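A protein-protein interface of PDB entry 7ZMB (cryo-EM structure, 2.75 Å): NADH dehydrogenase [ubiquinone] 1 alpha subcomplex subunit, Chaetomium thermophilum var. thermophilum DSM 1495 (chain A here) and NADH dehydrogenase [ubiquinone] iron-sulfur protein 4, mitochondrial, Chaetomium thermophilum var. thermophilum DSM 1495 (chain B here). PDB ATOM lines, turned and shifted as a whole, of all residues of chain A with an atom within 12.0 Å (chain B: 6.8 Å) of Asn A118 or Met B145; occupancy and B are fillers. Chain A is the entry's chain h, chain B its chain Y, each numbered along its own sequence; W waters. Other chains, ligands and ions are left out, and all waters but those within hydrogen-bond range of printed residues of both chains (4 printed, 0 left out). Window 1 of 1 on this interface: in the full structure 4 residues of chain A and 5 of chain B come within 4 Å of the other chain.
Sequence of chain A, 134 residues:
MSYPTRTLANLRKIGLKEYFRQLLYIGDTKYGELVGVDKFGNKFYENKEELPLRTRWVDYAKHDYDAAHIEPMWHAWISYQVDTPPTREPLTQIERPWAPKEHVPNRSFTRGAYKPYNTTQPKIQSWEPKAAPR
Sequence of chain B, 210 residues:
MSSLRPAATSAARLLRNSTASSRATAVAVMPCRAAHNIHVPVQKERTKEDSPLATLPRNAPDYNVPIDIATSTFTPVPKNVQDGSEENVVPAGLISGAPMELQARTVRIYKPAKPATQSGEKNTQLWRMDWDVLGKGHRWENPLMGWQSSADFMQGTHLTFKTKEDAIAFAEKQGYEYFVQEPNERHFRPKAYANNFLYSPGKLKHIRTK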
ATOM      1  N   TYR A 114      11.953  34.917   9.239  1.00  0.00           N
ATOM      2  CA  TYR A 114      11.128  34.029  10.094  1.00  0.00           C
ATOM      3  C   TYR A 114      11.706  32.621  10.116  1.00  0.00           C
ATOM      4  O   TYR A 114      12.053  32.063   9.060  1.00  0.00           O
ATOM      5  CB  TYR A 114       9.678  34.020   9.601  1.00  0.00           C
ATOM      6  CG  TYR A 114       8.839  32.834  10.002  1.00  0.00           C
ATOM      7  CD1 TYR A 114       8.429  32.654  11.311  1.00  0.00           C
ATOM      8  CD2 TYR A 114       8.424  31.911   9.059  1.00  0.00           C
ATOM      9  CE1 TYR A 114       7.646  31.576  11.683  1.00  0.00           C
ATOM     10  CE2 TYR A 114       7.641  30.827   9.411  1.00  0.00           C
ATOM     11  CZ  TYR A 114       7.248  30.661  10.727  1.00  0.00           C
ATOM     12  OH  TYR A 114       6.479  29.596  11.080  1.00  0.00           O
ATOM     13  N   LYS A 115      11.809  32.068  11.316  1.00  0.00           N
ATOM     14  CA  LYS A 115      12.275  30.678  11.467  1.00  0.00           C
ATOM     15  C   LYS A 115      11.073  29.907  12.010  1.00  0.00           C
ATOM     16  O   LYS A 115      10.577  30.278  13.080  1.00  0.00           O
ATOM     17  CB  LYS A 115      13.464  30.672  12.429  1.00  0.00           C
ATOM     18  CG  LYS A 115      14.596  31.642  12.120  1.00  0.00           C
ATOM     19  CD  LYS A 115      15.325  31.317  10.841  1.00  0.00           C
ATOM     20  CE  LYS A 115      16.580  32.137  10.643  1.00  0.00           C
ATOM     21  NZ  LYS A 115      17.708  31.603  11.440  1.00  0.00           N
ATOM     22  N   PRO A 116      10.595  28.850  11.330  1.00  0.00           N
ATOM     23  CA  PRO A 116       9.461  28.050  11.811  1.00  0.00           C
ATOM     24  C   PRO A 116       9.813  27.159  13.010  1.00  0.00           C
ATOM     25  O   PRO A 116      10.981  26.977  13.258  1.00  0.00           O
ATOM     26  CB  PRO A 116       9.163  27.176  10.589  1.00  0.00           C
ATOM     27  CG  PRO A 116      10.509  26.982   9.952  1.00  0.00           C
ATOM     28  CD  PRO A 116      11.134  28.353  10.066  1.00  0.00           C
ATOM     29  N   TYR A 117       8.820  26.676  13.755  1.00  0.00           N
ATOM     30  CA  TYR A 117       9.105  25.723  14.859  1.00  0.00           C
ATOM     31  C   TYR A 117       7.870  24.948  15.309  1.00  0.00           C
ATOM     32  O   TYR A 117       6.757  25.337  14.937  1.00  0.00           O
ATOM     33  CB  TYR A 117       9.685  26.416  16.095  1.00  0.00           C
ATOM     34  CG  TYR A 117       8.959  27.640  16.583  1.00  0.00           C
ATOM     35  CD1 TYR A 117       9.171  28.873  15.992  1.00  0.00           C
ATOM     36  CD2 TYR A 117       8.091  27.576  17.657  1.00  0.00           C
ATOM     37  CE1 TYR A 117       8.509  30.005  16.431  1.00  0.00           C
ATOM     38  CE2 TYR A 117       7.434  28.702  18.121  1.00  0.00           C
ATOM     39  CZ  TYR A 117       7.646  29.921  17.506  1.00  0.00           C
ATOM     40  OH  TYR A 117       7.013  31.041  17.950  1.00  0.00           O
ATOM     41  N   ASN A 118       8.080  23.873  16.072  1.00  0.00           N
ATOM     42  CA  ASN A 118       6.984  23.155  16.694  1.00  0.00           C
ATOM     43  C   ASN A 118       6.418  23.991  17.838  1.00  0.00           C
ATOM     44  O   ASN A 118       7.158  24.411  18.727  1.00  0.00           O
ATOM     45  CB  ASN A 118       7.501  21.810  17.198  1.00  0.00           C
ATOM     46  CG  ASN A 118       6.409  20.781  17.378  1.00  0.00           C
ATOM     47  OD1 ASN A 118       5.223  21.089  17.347  1.00  0.00           O
ATOM     48  ND2 ASN A 118       6.815  19.548  17.590  1.00  0.00           N
ATOM     49  N   THR A 119       5.115  24.245  17.814  1.00  0.00           N
ATOM     50  CA  THR A 119       4.447  24.945  18.901  1.00  0.00           C
ATOM     51  C   THR A 119       3.877  23.997  19.946  1.00  0.00           C
ATOM     52  O   THR A 119       3.238  24.453  20.894  1.00  0.00           O
ATOM     53  CB  THR A 119       3.322  25.836  18.357  1.00  0.00           C
ATOM     54  OG1 THR A 119       2.347  25.033  17.687  1.00  0.00           O
ATOM     55  CG2 THR A 119       3.866  26.867  17.391  1.00  0.00           C
ATOM     56  N   THR A 120       4.103  22.698  19.799  1.00  0.00           N
ATOM     57  CA  THR A 120       3.479  21.684  20.628  1.00  0.00           C
ATOM     58  C   THR A 120       4.563  20.891  21.349  1.00  0.00           C
ATOM     59  O   THR A 120       5.695  20.792  20.877  1.00  0.00           O
ATOM     60  CB  THR A 120       2.587  20.769  19.763  1.00  0.00           C
ATOM     61  OG1 THR A 120       1.573  21.556  19.132  1.00  0.00           O
ATOM     62  CG2 THR A 120       1.885  19.725  20.594  1.00  0.00           C
ATOM     63  N   GLN A 121       4.220  20.361  22.519  1.00  0.00           N
ATOM     64  CA  GLN A 121       5.112  19.508  23.286  1.00  0.00           C
ATOM     65  C   GLN A 121       5.251  18.138  22.633  1.00  0.00           C
ATOM     66  O   GLN A 121       4.434  17.755  21.795  1.00  0.00           O
ATOM     67  CB  GLN A 121       4.591  19.357  24.714  1.00  0.00           C
ATOM     68  CG  GLN A 121       4.702  20.610  25.572  1.00  0.00           C
ATOM     69  CD  GLN A 121       6.121  20.962  25.928  1.00  0.00           C
ATOM     70  OE1 GLN A 121       6.934  21.275  25.067  1.00  0.00           O
ATOM     71  NE2 GLN A 121       6.426  20.929  27.211  1.00  0.00           N
ATOM     72  N   PRO A 122       6.294  17.388  22.978  1.00  0.00           N
ATOM     73  CA  PRO A 122       6.419  16.025  22.453  1.00  0.00           C
ATOM     74  C   PRO A 122       5.274  15.138  22.918  1.00  0.00           C
ATOM     75  O   PRO A 122       4.605  15.415  23.916  1.00  0.00           O
ATOM     76  CB  PRO A 122       7.766  15.552  23.012  1.00  0.00           C
ATOM     77  CG  PRO A 122       8.034  16.440  24.158  1.00  0.00           C
ATOM     78  CD  PRO A 122       7.482  17.767  23.755  1.00  0.00           C
ATOM     79  N   LYS A 123       5.053  14.058  22.174  1.00  0.00           N
ATOM     80  CA  LYS A 123       3.816  13.304  22.331  1.00  0.00           C
ATOM     81  C   LYS A 123       3.965  12.157  23.322  1.00  0.00           C
ATOM     82  O   LYS A 123       2.975  11.703  23.903  1.00  0.00           O
ATOM     83  CB  LYS A 123       3.345  12.802  20.968  1.00  0.00           C
ATOM     84  CG  LYS A 123       3.162  13.930  19.972  1.00  0.00           C
ATOM     85  CD  LYS A 123       1.943  13.743  19.114  1.00  0.00           C
ATOM     86  CE  LYS A 123       2.005  14.641  17.892  1.00  0.00           C
ATOM     87  NZ  LYS A 123       2.099  16.077  18.262  1.00  0.00           N
ATOM     88  N   ILE A 124       5.184  11.684  23.546  1.00  0.00           N
ATOM     89  CA  ILE A 124       5.439  10.587  24.469  1.00  0.00           C
ATOM     90  C   ILE A 124       6.562  10.998  25.414  1.00  0.00           C
ATOM     91  O   ILE A 124       7.587  11.530  24.979  1.00  0.00           O
ATOM     92  CB  ILE A 124       5.763   9.283  23.713  1.00  0.00           C
ATOM     93  CG1 ILE A 124       5.781   8.096  24.667  1.00  0.00           C
ATOM     94  CG2 ILE A 124       7.063   9.395  22.936  1.00  0.00           C
ATOM     95  CD1 ILE A 124       5.771   6.773  23.969  1.00  0.00           C
ATOM     96  N   GLN A 125       6.352  10.781  26.704  1.00  0.00           N
ATOM     97  CA  GLN A 125       7.319  11.143  27.732  1.00  0.00           C
ATOM     98  C   GLN A 125       7.958   9.886  28.297  1.00  0.00           C
ATOM     99  O   GLN A 125       7.257   8.975  28.746  1.00  0.00           O
ATOM    100  CB  GLN A 125       6.654  11.935  28.855  1.00  0.00           C
ATOM    101  CG  GLN A 125       5.968  13.207  28.403  1.00  0.00           C
ATOM    102  CD  GLN A 125       6.938  14.355  28.212  1.00  0.00           C
ATOM    103  OE1 GLN A 125       7.851  14.283  27.389  1.00  0.00           O
ATOM    104  NE2 GLN A 125       6.746  15.424  28.975  1.00  0.00           N
ATOM    105  N   GLU B 141       8.157  11.740  14.580  1.00  0.00           N
ATOM    106  CA  GLU B 141       7.964  13.208  14.561  1.00  0.00           C
ATOM    107  C   GLU B 141       9.080  13.942  13.822  1.00  0.00           C
ATOM    108  O   GLU B 141      10.250  13.710  14.137  1.00  0.00           O
ATOM    109  CB  GLU B 141       7.823  13.704  15.997  1.00  0.00           C
ATOM    110  CG  GLU B 141       7.565  15.188  16.120  1.00  0.00           C
ATOM    111  CD  GLU B 141       7.916  15.739  17.488  1.00  0.00           C
ATOM    112  OE1 GLU B 141       8.647  15.054  18.230  1.00  0.00           O
ATOM    113  OE2 GLU B 141       7.460  16.847  17.808  1.00  0.00           O
ATOM    114  N   ASN B 142       8.706  14.790  12.866  1.00  0.00           N
ATOM    115  CA  ASN B 142       9.656  15.605  12.122  1.00  0.00           C
ATOM    116  C   ASN B 142      10.356  16.579  13.063  1.00  0.00           C
ATOM    117  O   ASN B 142       9.690  17.239  13.869  1.00  0.00           O
ATOM    118  CB  ASN B 142       8.914  16.363  11.021  1.00  0.00           C
ATOM    119  CG  ASN B 142       9.832  17.160  10.109  1.00  0.00           C
ATOM    120  OD1 ASN B 142       9.621  18.341   9.845  1.00  0.00           O
ATOM    121  ND2 ASN B 142      10.876  16.503   9.634  1.00  0.00           N
ATOM    122  N   PRO B 143      11.682  16.698  13.000  1.00  0.00           N
ATOM    123  CA  PRO B 143      12.376  17.640  13.895  1.00  0.00           C
ATOM    124  C   PRO B 143      11.976  19.090  13.688  1.00  0.00           C
ATOM    125  O   PRO B 143      12.067  19.885  14.628  1.00  0.00           O
ATOM    126  CB  PRO B 143      13.856  17.425  13.561  1.00  0.00           C
ATOM    127  CG  PRO B 143      13.920  16.211  12.734  1.00  0.00           C
ATOM    128  CD  PRO B 143      12.606  15.989  12.105  1.00  0.00           C
ATOM    129  N   LEU B 144      11.539  19.459  12.487  1.00  0.00           N
ATOM    130  CA  LEU B 144      11.303  20.861  12.166  1.00  0.00           C
ATOM    131  C   LEU B 144       9.974  21.362  12.720  1.00  0.00           C
ATOM    132  O   LEU B 144       9.937  22.280  13.543  1.00  0.00           O
ATOM    133  CB  LEU B 144      11.353  21.056  10.651  1.00  0.00           C
ATOM    134  CG  LEU B 144      11.524  22.482  10.142  1.00  0.00           C
ATOM    135  CD1 LEU B 144      12.771  23.101  10.710  1.00  0.00           C
ATOM    136  CD2 LEU B 144      11.581  22.484   8.639  1.00  0.00           C
ATOM    137  N   MET B 145       8.868  20.775  12.268  1.00  0.00           N
ATOM    138  CA  MET B 145       7.539  21.326  12.630  1.00  0.00           C
ATOM    139  C   MET B 145       6.793  20.454  13.620  1.00  0.00           C
ATOM    140  O   MET B 145       5.844  20.959  14.185  1.00  0.00           O
ATOM    141  CB  MET B 145       6.693  21.403  11.357  1.00  0.00           C
ATOM    142  CG  MET B 145       7.171  22.458  10.381  1.00  0.00           C
ATOM    143  SD  MET B 145       7.283  24.088  11.156  1.00  0.00           S
ATOM    144  CE  MET B 145       5.628  24.711  10.876  1.00  0.00           C
ATOM    145  N   GLY B 146       7.264  19.248  13.893  1.00  0.00           N
ATOM    146  CA  GLY B 146       6.478  18.315  14.664  1.00  0.00           C
ATOM    147  C   GLY B 146       5.436  17.561  13.876  1.00  0.00           C
ATOM    148  O   GLY B 146       4.638  16.842  14.480  1.00  0.00           O
ATOM    149  N   TRP B 147       5.407  17.708  12.552  1.00  0.00           N
ATOM    150  CA  TRP B 147       4.540  16.885  11.729  1.00  0.00           C
ATOM    151  C   TRP B 147       4.950  15.423  11.845  1.00  0.00           C
ATOM    152  O   TRP B 147       6.086  15.092  12.190  1.00  0.00           O
ATOM    153  CB  TRP B 147       4.597  17.309  10.262  1.00  0.00           C
ATOM    154  CG  TRP B 147       4.153  18.697   9.988  1.00  0.00           C
ATOM    155  CD1 TRP B 147       3.341  19.467  10.760  1.00  0.00           C
ATOM    156  CD2 TRP B 147       4.504  19.492   8.857  1.00  0.00           C
ATOM    157  NE1 TRP B 147       3.165  20.694  10.180  1.00  0.00           N
ATOM    158  CE2 TRP B 147       3.871  20.734   9.009  1.00  0.00           C
ATOM    159  CE3 TRP B 147       5.304  19.276   7.735  1.00  0.00           C
ATOM    160  CZ2 TRP B 147       4.009  21.759   8.075  1.00  0.00           C
ATOM    161  CZ3 TRP B 147       5.439  20.288   6.814  1.00  0.00           C
ATOM    162  CH2 TRP B 147       4.794  21.512   6.983  1.00  0.00           C
HETATM  163  O   HOH W   1       7.017  13.226  19.941  1.00  0.00           O
HETATM  164  O   HOH W   2       5.277  17.699  18.995  1.00  0.00           O
HETATM  165  O   HOH W   3       9.858  19.359  16.827  1.00  0.00           O
HETATM  166  O   HOH W   4      11.140  23.368  16.298  1.00  0.00           O
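The side-chain carboxylate of Glu B141 lies within hydrogen-bond range of the side-chain amide nitrogen of Asn A118, 2.8 Å away.
O of Met B145 lies close to OD1 of Asn A118.
Asn A118 touches just these residues of chain B: Glu B141 (2.8 Å), Leu B144 (3.5 Å), Met B145 (3.2 Å) and Gly B146 (3.2 Å).
Met B145 touches three residues of chain A.
No residue of chain A comes within 4 Å of Asn B142.
No residue of chain A comes within 4 Å of Pro B143.
Leu B144 touches just these residues of chain A: Tyr A117 (3.8 Å) and Asn A118 (3.5 Å).
No residue of chain A comes within 4 Å of Trp B147.
Printed residues of chain A within 4 Å of Glu B141: Asn A118 (2.8 Å).
Printed residues of chain B within 4 Å of Tyr A117: Leu B144 (3.8 Å) and Met B145 (3.98 Å).
Printed residues of chain B within 4 Å of Pro A116: Met B145 (3.7 Å).
Gln A125 touches none of the printed residues of chain B.
The nearest residue of chain B that does not touch Asn A118 is Asn B142 (5.2 Å).
The nearest printed residue of chain A that does not touch Met B145 is Thr A119 (4.9 Å).
Among the printed residues, merely in contact across the chains: Asn A118 with Gly B146 (3.2 Å), Asn A118 with Leu B144 (3.5 Å), Pro A116 with Met B145 (3.7 Å), Tyr A117 with Leu B144 (3.8 Å) and Tyr A117 with Met B145 (3.98 Å).
Of the 7 printed residues of chain B, 4 touch a printed residue of chain A.
Among the printed residues, 7 pairs touch across the chains.
Among the printed residues, no Asp or Glu carboxylate lies within 4 Å of a Lys or Arg side-chain nitrogen of the other chain.
The side-chain amide oxygen (OD1) of Asn B142 lies close to the backbone NH (N) of Leu B144 (3.5 Å).
OD1 of Asn A118 lies within hydrogen-bond range of N of Thr A120 (3.1 Å).
Water W2 lies within hydrogen-bond range of the side-chain carboxylate of Glu B141, the side-chain amide nitrogen of Asn A118 and the backbone carbonyl oxygen of Gln A121.
Water W1 bridges the side-chain carboxylate (OE1) of Glu B141 (3.0 Å) and the backbone NH (N) of Lys A123 (3.1 Å).
Water W4 lies within hydrogen-bond range of the backbone NH of Asn A118 (3.1 Å) and the backbone carbonyl oxygen of Leu B144 (3.2 Å).
Water W3 bridges the side-chain amide nitrogen of Asn A118 (3.1 Å) and the backbone carbonyl oxygen of Pro B143 (3.2 Å).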
